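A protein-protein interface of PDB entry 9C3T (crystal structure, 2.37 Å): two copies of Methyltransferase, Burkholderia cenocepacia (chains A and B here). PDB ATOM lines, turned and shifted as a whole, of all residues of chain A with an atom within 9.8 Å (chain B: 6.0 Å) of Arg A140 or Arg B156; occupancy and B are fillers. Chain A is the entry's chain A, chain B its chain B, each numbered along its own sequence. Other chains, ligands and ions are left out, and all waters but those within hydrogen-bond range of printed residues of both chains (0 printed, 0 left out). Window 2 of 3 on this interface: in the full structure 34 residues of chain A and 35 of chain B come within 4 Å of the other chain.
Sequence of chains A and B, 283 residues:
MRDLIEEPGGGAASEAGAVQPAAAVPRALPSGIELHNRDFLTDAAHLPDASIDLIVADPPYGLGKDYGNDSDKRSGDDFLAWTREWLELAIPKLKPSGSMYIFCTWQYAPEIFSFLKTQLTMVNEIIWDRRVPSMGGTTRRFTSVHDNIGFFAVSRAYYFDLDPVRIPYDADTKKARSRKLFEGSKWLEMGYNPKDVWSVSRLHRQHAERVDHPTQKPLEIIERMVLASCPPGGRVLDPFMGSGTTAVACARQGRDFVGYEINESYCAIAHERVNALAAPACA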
ATOM      1  N   GLY A 136      20.141  13.836   6.968  1.00  0.00           N
ATOM      2  CA  GLY A 136      19.121  14.396   7.863  1.00  0.00           C
ATOM      3  C   GLY A 136      17.842  13.597   7.809  1.00  0.00           C
ATOM      4  O   GLY A 136      17.440  13.075   8.854  1.00  0.00           O
ATOM      5  N   GLY A 137      17.216  13.524   6.638  1.00  0.00           N
ATOM      6  CA  GLY A 137      15.978  12.751   6.471  1.00  0.00           C
ATOM      7  C   GLY A 137      14.881  13.539   5.791  1.00  0.00           C
ATOM      8  O   GLY A 137      13.742  13.044   5.769  1.00  0.00           O
ATOM      9  N   THR A 138      15.197  14.706   5.239  1.00  0.00           N
ATOM     10  CA  THR A 138      14.153  15.568   4.645  1.00  0.00           C
ATOM     11  C   THR A 138      13.665  15.024   3.327  1.00  0.00           C
ATOM     12  O   THR A 138      14.418  14.286   2.674  1.00  0.00           O
ATOM     13  CB  THR A 138      14.648  17.002   4.489  1.00  0.00           C
ATOM     14  OG1 THR A 138      13.628  17.679   3.770  1.00  0.00           O
ATOM     15  CG2 THR A 138      15.957  17.091   3.727  1.00  0.00           C
ATOM     16  N   THR A 139      12.437  15.388   2.957  1.00  0.00           N
ATOM     17  CA  THR A 139      11.848  15.008   1.665  1.00  0.00           C
ATOM     18  C   THR A 139      11.068  16.212   1.184  1.00  0.00           C
ATOM     19  O   THR A 139      10.400  16.094   0.159  1.00  0.00           O
ATOM     20  CB  THR A 139      10.985  13.759   1.837  1.00  0.00           C
ATOM     21  OG1 THR A 139      10.503  13.771   3.175  1.00  0.00           O
ATOM     22  CG2 THR A 139      11.758  12.475   1.604  1.00  0.00           C
ATOM     23  N   ARG A 140      11.183  17.342   1.880  1.00  0.00           N
ATOM     24  CA  ARG A 140      10.394  18.560   1.565  1.00  0.00           C
ATOM     25  C   ARG A 140      11.260  19.653   0.939  1.00  0.00           C
ATOM     26  O   ARG A 140      10.767  20.782   0.821  1.00  0.00           O
ATOM     27  CB  ARG A 140       9.796  19.138   2.849  1.00  0.00           C
ATOM     28  CG  ARG A 140       8.977  18.171   3.689  1.00  0.00           C
ATOM     29  CD  ARG A 140       7.519  18.580   3.803  1.00  0.00           C
ATOM     30  NE  ARG A 140       7.334  20.017   4.025  1.00  0.00           N
ATOM     31  CZ  ARG A 140       6.642  20.812   3.226  1.00  0.00           C
ATOM     32  NH1 ARG A 140       6.144  20.341   2.102  1.00  0.00           N
ATOM     33  NH2 ARG A 140       6.450  22.071   3.554  1.00  0.00           N
ATOM     34  N   ARG A 141      12.485  19.329   0.552  1.00  0.00           N
ATOM     35  CA  ARG A 141      13.413  20.280  -0.047  1.00  0.00           C
ATOM     36  C   ARG A 141      14.544  19.485  -0.680  1.00  0.00           C
ATOM     37  O   ARG A 141      14.783  18.328  -0.324  1.00  0.00           O
ATOM     38  CB  ARG A 141      13.964  21.270   0.987  1.00  0.00           C
ATOM     39  CG  ARG A 141      15.233  20.778   1.670  1.00  0.00           C
ATOM     40  CD  ARG A 141      15.690  21.675   2.815  1.00  0.00           C
ATOM     41  NE  ARG A 141      15.328  23.079   2.665  1.00  0.00           N
ATOM     42  CZ  ARG A 141      14.918  23.850   3.664  1.00  0.00           C
ATOM     43  NH1 ARG A 141      14.735  23.364   4.882  1.00  0.00           N
ATOM     44  NH2 ARG A 141      14.684  25.139   3.439  1.00  0.00           N
ATOM     45  N   PHE A 142      15.253  20.120  -1.615  1.00  0.00           N
ATOM     46  CA  PHE A 142      16.410  19.474  -2.287  1.00  0.00           C
ATOM     47  C   PHE A 142      17.551  19.424  -1.292  1.00  0.00           C
ATOM     48  O   PHE A 142      17.638  20.304  -0.435  1.00  0.00           O
ATOM     49  CB  PHE A 142      16.700  20.201  -3.602  1.00  0.00           C
ATOM     50  CG  PHE A 142      15.552  20.211  -4.605  1.00  0.00           C
ATOM     51  CD1 PHE A 142      15.289  19.107  -5.403  1.00  0.00           C
ATOM     52  CD2 PHE A 142      14.743  21.329  -4.752  1.00  0.00           C
ATOM     53  CE1 PHE A 142      14.249  19.122  -6.314  1.00  0.00           C
ATOM     54  CE2 PHE A 142      13.704  21.336  -5.666  1.00  0.00           C
ATOM     55  CZ  PHE A 142      13.459  20.233  -6.442  1.00  0.00           C
ATOM     56  N   THR A 143      18.417  18.431  -1.411  1.00  0.00           N
ATOM     57  CA  THR A 143      19.469  18.235  -0.397  1.00  0.00           C
ATOM     58  C   THR A 143      20.667  19.149  -0.602  1.00  0.00           C
ATOM     59  O   THR A 143      21.037  19.376  -1.752  1.00  0.00           O
ATOM     60  CB  THR A 143      19.839  16.751  -0.397  1.00  0.00           C
ATOM     61  OG1 THR A 143      19.738  16.284  -1.735  1.00  0.00           O
ATOM     62  CG2 THR A 143      18.924  15.935   0.497  1.00  0.00           C
ATOM     63  N   PRO B  96      -1.432  30.379  -0.549  1.00  0.00           N
ATOM     64  CA  PRO B  96      -0.589  30.134   0.638  1.00  0.00           C
ATOM     65  C   PRO B  96       0.332  28.935   0.510  1.00  0.00           C
ATOM     66  O   PRO B  96       1.433  28.949   1.075  1.00  0.00           O
ATOM     67  CB  PRO B  96      -1.603  29.943   1.779  1.00  0.00           C
ATOM     68  CG  PRO B  96      -2.924  29.785   1.162  1.00  0.00           C
ATOM     69  CD  PRO B  96      -2.873  30.336  -0.228  1.00  0.00           C
ATOM     70  N   THR B 121       9.893  32.929   2.215  1.00  0.00           N
ATOM     71  CA  THR B 121      10.876  32.122   2.959  1.00  0.00           C
ATOM     72  C   THR B 121      11.682  31.327   1.961  1.00  0.00           C
ATOM     73  O   THR B 121      11.085  30.694   1.085  1.00  0.00           O
ATOM     74  CB  THR B 121      10.166  31.203   3.951  1.00  0.00           C
ATOM     75  OG1 THR B 121       9.575  32.078   4.903  1.00  0.00           O
ATOM     76  CG2 THR B 121      11.104  30.221   4.626  1.00  0.00           C
ATOM     77  N   VAL B 123      13.632  28.217   0.707  1.00  0.00           N
ATOM     78  CA  VAL B 123      13.649  26.765   1.006  1.00  0.00           C
ATOM     79  C   VAL B 123      14.965  26.213   0.450  1.00  0.00           C
ATOM     80  O   VAL B 123      15.539  25.321   1.079  1.00  0.00           O
ATOM     81  CB  VAL B 123      12.410  26.059   0.423  1.00  0.00           C
ATOM     82  CG1 VAL B 123      12.433  24.554   0.630  1.00  0.00           C
ATOM     83  CG2 VAL B 123      11.117  26.677   0.930  1.00  0.00           C
ATOM     84  N   ASN B 124      15.423  26.754  -0.670  1.00  0.00           N
ATOM     85  CA  ASN B 124      16.645  26.201  -1.291  1.00  0.00           C
ATOM     86  C   ASN B 124      17.316  27.162  -2.267  1.00  0.00           C
ATOM     87  O   ASN B 124      16.648  28.067  -2.776  1.00  0.00           O
ATOM     88  CB  ASN B 124      16.361  24.922  -2.068  1.00  0.00           C
ATOM     89  CG  ASN B 124      16.559  23.653  -1.282  1.00  0.00           C
ATOM     90  OD1 ASN B 124      15.757  22.726  -1.413  1.00  0.00           O
ATOM     91  ND2 ASN B 124      17.610  23.581  -0.482  1.00  0.00           N
ATOM     92  N   PHE B 151      14.609  29.080  -4.611  1.00  0.00           N
ATOM     93  CA  PHE B 151      13.367  28.341  -4.284  1.00  0.00           C
ATOM     94  C   PHE B 151      12.779  28.986  -3.055  1.00  0.00           C
ATOM     95  O   PHE B 151      13.250  28.764  -1.941  1.00  0.00           O
ATOM     96  CB  PHE B 151      13.692  26.855  -4.132  1.00  0.00           C
ATOM     97  CG  PHE B 151      12.490  25.953  -3.900  1.00  0.00           C
ATOM     98  CD1 PHE B 151      11.242  26.282  -4.412  1.00  0.00           C
ATOM     99  CD2 PHE B 151      12.616  24.784  -3.164  1.00  0.00           C
ATOM    100  CE1 PHE B 151      10.155  25.458  -4.196  1.00  0.00           C
ATOM    101  CE2 PHE B 151      11.523  23.965  -2.953  1.00  0.00           C
ATOM    102  CZ  PHE B 151      10.299  24.304  -3.467  1.00  0.00           C
ATOM    103  N   ALA B 153       9.180  30.027  -0.772  1.00  0.00           N
ATOM    104  CA  ALA B 153       7.789  29.615  -0.495  1.00  0.00           C
ATOM    105  C   ALA B 153       7.076  30.715   0.287  1.00  0.00           C
ATOM    106  O   ALA B 153       7.739  31.470   1.000  1.00  0.00           O
ATOM    107  CB  ALA B 153       7.789  28.324   0.265  1.00  0.00           C
ATOM    108  N   VAL B 154       5.753  30.773   0.170  1.00  0.00           N
ATOM    109  CA  VAL B 154       4.951  31.834   0.853  1.00  0.00           C
ATOM    110  C   VAL B 154       4.855  31.490   2.341  1.00  0.00           C
ATOM    111  O   VAL B 154       5.035  32.386   3.173  1.00  0.00           O
ATOM    112  CB  VAL B 154       3.557  31.976   0.217  1.00  0.00           C
ATOM    113  CG1 VAL B 154       2.821  33.204   0.725  1.00  0.00           C
ATOM    114  CG2 VAL B 154       3.621  31.966  -1.302  1.00  0.00           C
ATOM    115  N   SER B 155       4.631  30.217   2.634  1.00  0.00           N
ATOM    116  CA  SER B 155       4.470  29.787   4.038  1.00  0.00           C
ATOM    117  C   SER B 155       5.195  28.463   4.257  1.00  0.00           C
ATOM    118  O   SER B 155       5.766  27.927   3.299  1.00  0.00           O
ATOM    119  CB  SER B 155       3.030  29.661   4.394  1.00  0.00           C
ATOM    120  OG  SER B 155       2.188  29.879   3.273  1.00  0.00           O
ATOM    121  N   ARG B 156       5.145  27.968   5.483  1.00  0.00           N
ATOM    122  CA  ARG B 156       5.854  26.739   5.805  1.00  0.00           C
ATOM    123  C   ARG B 156       5.102  25.496   5.353  1.00  0.00           C
ATOM    124  O   ARG B 156       5.677  24.402   5.379  1.00  0.00           O
ATOM    125  CB  ARG B 156       6.117  26.681   7.310  1.00  0.00           C
ATOM    126  CG  ARG B 156       6.535  28.019   7.898  1.00  0.00           C
ATOM    127  CD  ARG B 156       6.163  28.126   9.365  1.00  0.00           C
ATOM    128  NE  ARG B 156       6.719  27.028  10.148  1.00  0.00           N
ATOM    129  CZ  ARG B 156       6.720  26.981  11.472  1.00  0.00           C
ATOM    130  NH1 ARG B 156       6.206  27.959  12.199  1.00  0.00           N
ATOM    131  NH2 ARG B 156       7.252  25.926  12.083  1.00  0.00           N
ATOM    132  N   ALA B 157       3.842  25.637   4.940  1.00  0.00           N
ATOM    133  CA  ALA B 157       3.039  24.529   4.438  1.00  0.00           C
ATOM    134  C   ALA B 157       3.044  24.455   2.915  1.00  0.00           C
ATOM    135  O   ALA B 157       2.058  24.022   2.310  1.00  0.00           O
ATOM    136  CB  ALA B 157       1.608  24.636   4.962  1.00  0.00           C
ATOM    137  N   TYR B 158       4.142  24.871   2.284  1.00  0.00           N
ATOM    138  CA  TYR B 158       4.221  24.867   0.830  1.00  0.00           C
ATOM    139  C   TYR B 158       4.106  23.448   0.288  1.00  0.00           C
ATOM    140  O   TYR B 158       4.602  22.492   0.889  1.00  0.00           O
ATOM    141  CB  TYR B 158       5.536  25.496   0.367  1.00  0.00           C
ATOM    142  CG  TYR B 158       6.777  24.830   0.926  1.00  0.00           C
ATOM    143  CD1 TYR B 158       7.309  25.220   2.150  1.00  0.00           C
ATOM    144  CD2 TYR B 158       7.419  23.815   0.227  1.00  0.00           C
ATOM    145  CE1 TYR B 158       8.441  24.615   2.662  1.00  0.00           C
ATOM    146  CE2 TYR B 158       8.550  23.203   0.733  1.00  0.00           C
ATOM    147  CZ  TYR B 158       9.057  23.607   1.949  1.00  0.00           C
ATOM    148  OH  TYR B 158      10.183  23.000   2.452  1.00  0.00           O
ATOM    149  N   TYR B 159       3.445  23.317  -0.857  1.00  0.00           N
ATOM    150  CA  TYR B 159       3.333  22.014  -1.496  1.00  0.00           C
ATOM    151  C   TYR B 159       4.683  21.596  -2.062  1.00  0.00           C
ATOM    152  O   TYR B 159       5.361  22.385  -2.729  1.00  0.00           O
ATOM    153  CB  TYR B 159       2.289  22.045  -2.609  1.00  0.00           C
ATOM    154  CG  TYR B 159       2.303  20.794  -3.455  1.00  0.00           C
ATOM    155  CD1 TYR B 159       1.747  19.609  -2.985  1.00  0.00           C
ATOM    156  CD2 TYR B 159       2.899  20.787  -4.708  1.00  0.00           C
ATOM    157  CE1 TYR B 159       1.767  18.461  -3.750  1.00  0.00           C
ATOM    158  CE2 TYR B 159       2.928  19.643  -5.477  1.00  0.00           C
ATOM    159  CZ  TYR B 159       2.359  18.484  -4.995  1.00  0.00           C
ATOM    160  OH  TYR B 159       2.382  17.341  -5.760  1.00  0.00           O
ATOM    161  N   PHE B 160       5.069  20.351  -1.802  1.00  0.00           N
ATOM    162  CA  PHE B 160       6.311  19.807  -2.342  1.00  0.00           C
ATOM    163  C   PHE B 160       6.193  18.294  -2.366  1.00  0.00           C
ATOM    164  O   PHE B 160       5.958  17.676  -1.323  1.00  0.00           O
ATOM    165  CB  PHE B 160       7.516  20.247  -1.510  1.00  0.00           C
ATOM    166  CG  PHE B 160       8.836  19.833  -2.093  1.00  0.00           C
ATOM    167  CD1 PHE B 160       9.495  20.643  -3.002  1.00  0.00           C
ATOM    168  CD2 PHE B 160       9.414  18.627  -1.737  1.00  0.00           C
ATOM    169  CE1 PHE B 160      10.710  20.258  -3.539  1.00  0.00           C
ATOM    170  CE2 PHE B 160      10.626  18.238  -2.269  1.00  0.00           C
ATOM    171  CZ  PHE B 160      11.274  19.053  -3.172  1.00  0.00           C
ATOM    172  N   LEU B 162       8.397  14.982  -3.691  1.00  0.00           N
ATOM    173  CA  LEU B 162       9.724  14.598  -4.225  1.00  0.00           C
ATOM    174  C   LEU B 162       9.637  13.313  -5.054  1.00  0.00           C
ATOM    175  O   LEU B 162      10.481  13.122  -5.933  1.00  0.00           O
ATOM    176  CB  LEU B 162      10.714  14.455  -3.068  1.00  0.00           C
ATOM    177  CG  LEU B 162      12.129  13.995  -3.423  1.00  0.00           C
ATOM    178  CD1 LEU B 162      13.018  15.199  -3.647  1.00  0.00           C
ATOM    179  CD2 LEU B 162      12.680  13.107  -2.329  1.00  0.00           C
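Hydrophobic or aromatic side chains of chain A within 4 Å of the printed part of chain B: Phe A142. Along chain A the printed residues that touch a printed residue of chain B span positions 139 to 142. Printed residues of chain B that touch a printed residue of chain A: Val B123, Asn B124, Arg B156, Tyr B158, Phe B160 and Leu B162. Hydrophobic or aromatic side chains of chain B that line the printed part of chain A: Val B123, Tyr B158, Phe B160 and Leu B162.
No position is printed for both chains.
O of Asn B124 is in hydrogen-bond range of N of Phe B151 (2.9 Å). The backbone NH (N) of Val B123 sits at hydrogen-bond distance from the backbone carbonyl oxygen (O) of Phe B151 (2.7 Å). The side-chain hydroxyl of Thr A138 is in hydrogen-bond range of the backbone NH of Arg A140, at 3.1 Å.
The guanidinium group (NH2) of Arg A140 sits at hydrogen-bond distance from the backbone carbonyl oxygen (O) of Arg B156 (3.1 Å). O of Val B123 lies within hydrogen-bond range of NH2 of Arg A141 (2.5 Å). The backbone carbonyl oxygen of Arg A140 sits at hydrogen-bond distance from the side-chain hydroxyl of Tyr B158 (2.8 Å). The backbone NH (N) of Phe A142 sits at hydrogen-bond distance from the side-chain amide oxygen (OD1) of Asn B124.
Printed residues of chain B within 4 Å of Thr A139: Phe B160 (3.2 Å) and Leu B162 (3.6 Å). Of chain B, only Arg B156 (3.1 Å), Tyr B158 (2.8 Å) and Phe B160 (3.4 Å) come within 4 Å of Arg A140. Of the printed residues of chain B, Arg A141 touches Val B123 (2.5 Å), Asn B124 (3.3 Å) and Phe B160 (3.6 Å). Of the printed residues of chain B, Phe A142 touches Asn B124 (2.7 Å) and Phe B160 (3.8 Å). Ser B155 touches none of the printed residues of chain A. Arg B156 touches just one residue of chain A: Arg A140. Of chain A, only Thr A139, Arg A140, Arg A141 and Phe A142 come within 4 Å of Phe B160. Of the printed residues of chain A, Leu B162 touches Thr A139 (3.6 Å). The nearest residue of chain B that does not touch Arg A140 is Val B123 (4.1 Å). The nearest residue of chain A that does not touch Arg B156 is Arg A141 (9.1 Å). The nearest printed residue of chain A that does not touch Asn B124 is Thr A143 (5.1 Å).
Thr A139 touches Phe B160 (O to CE2, 3.2 Å). O of Thr A139 touches CB of Leu B162, 3.6 Å away. Arg A140 touches Phe B160 (C to CD2, 3.4 Å). Asn B124 touches Arg A141. N of Arg A141 touches CE2 of Phe B160, at 3.6 Å. Phe B160 touches Phe A142.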
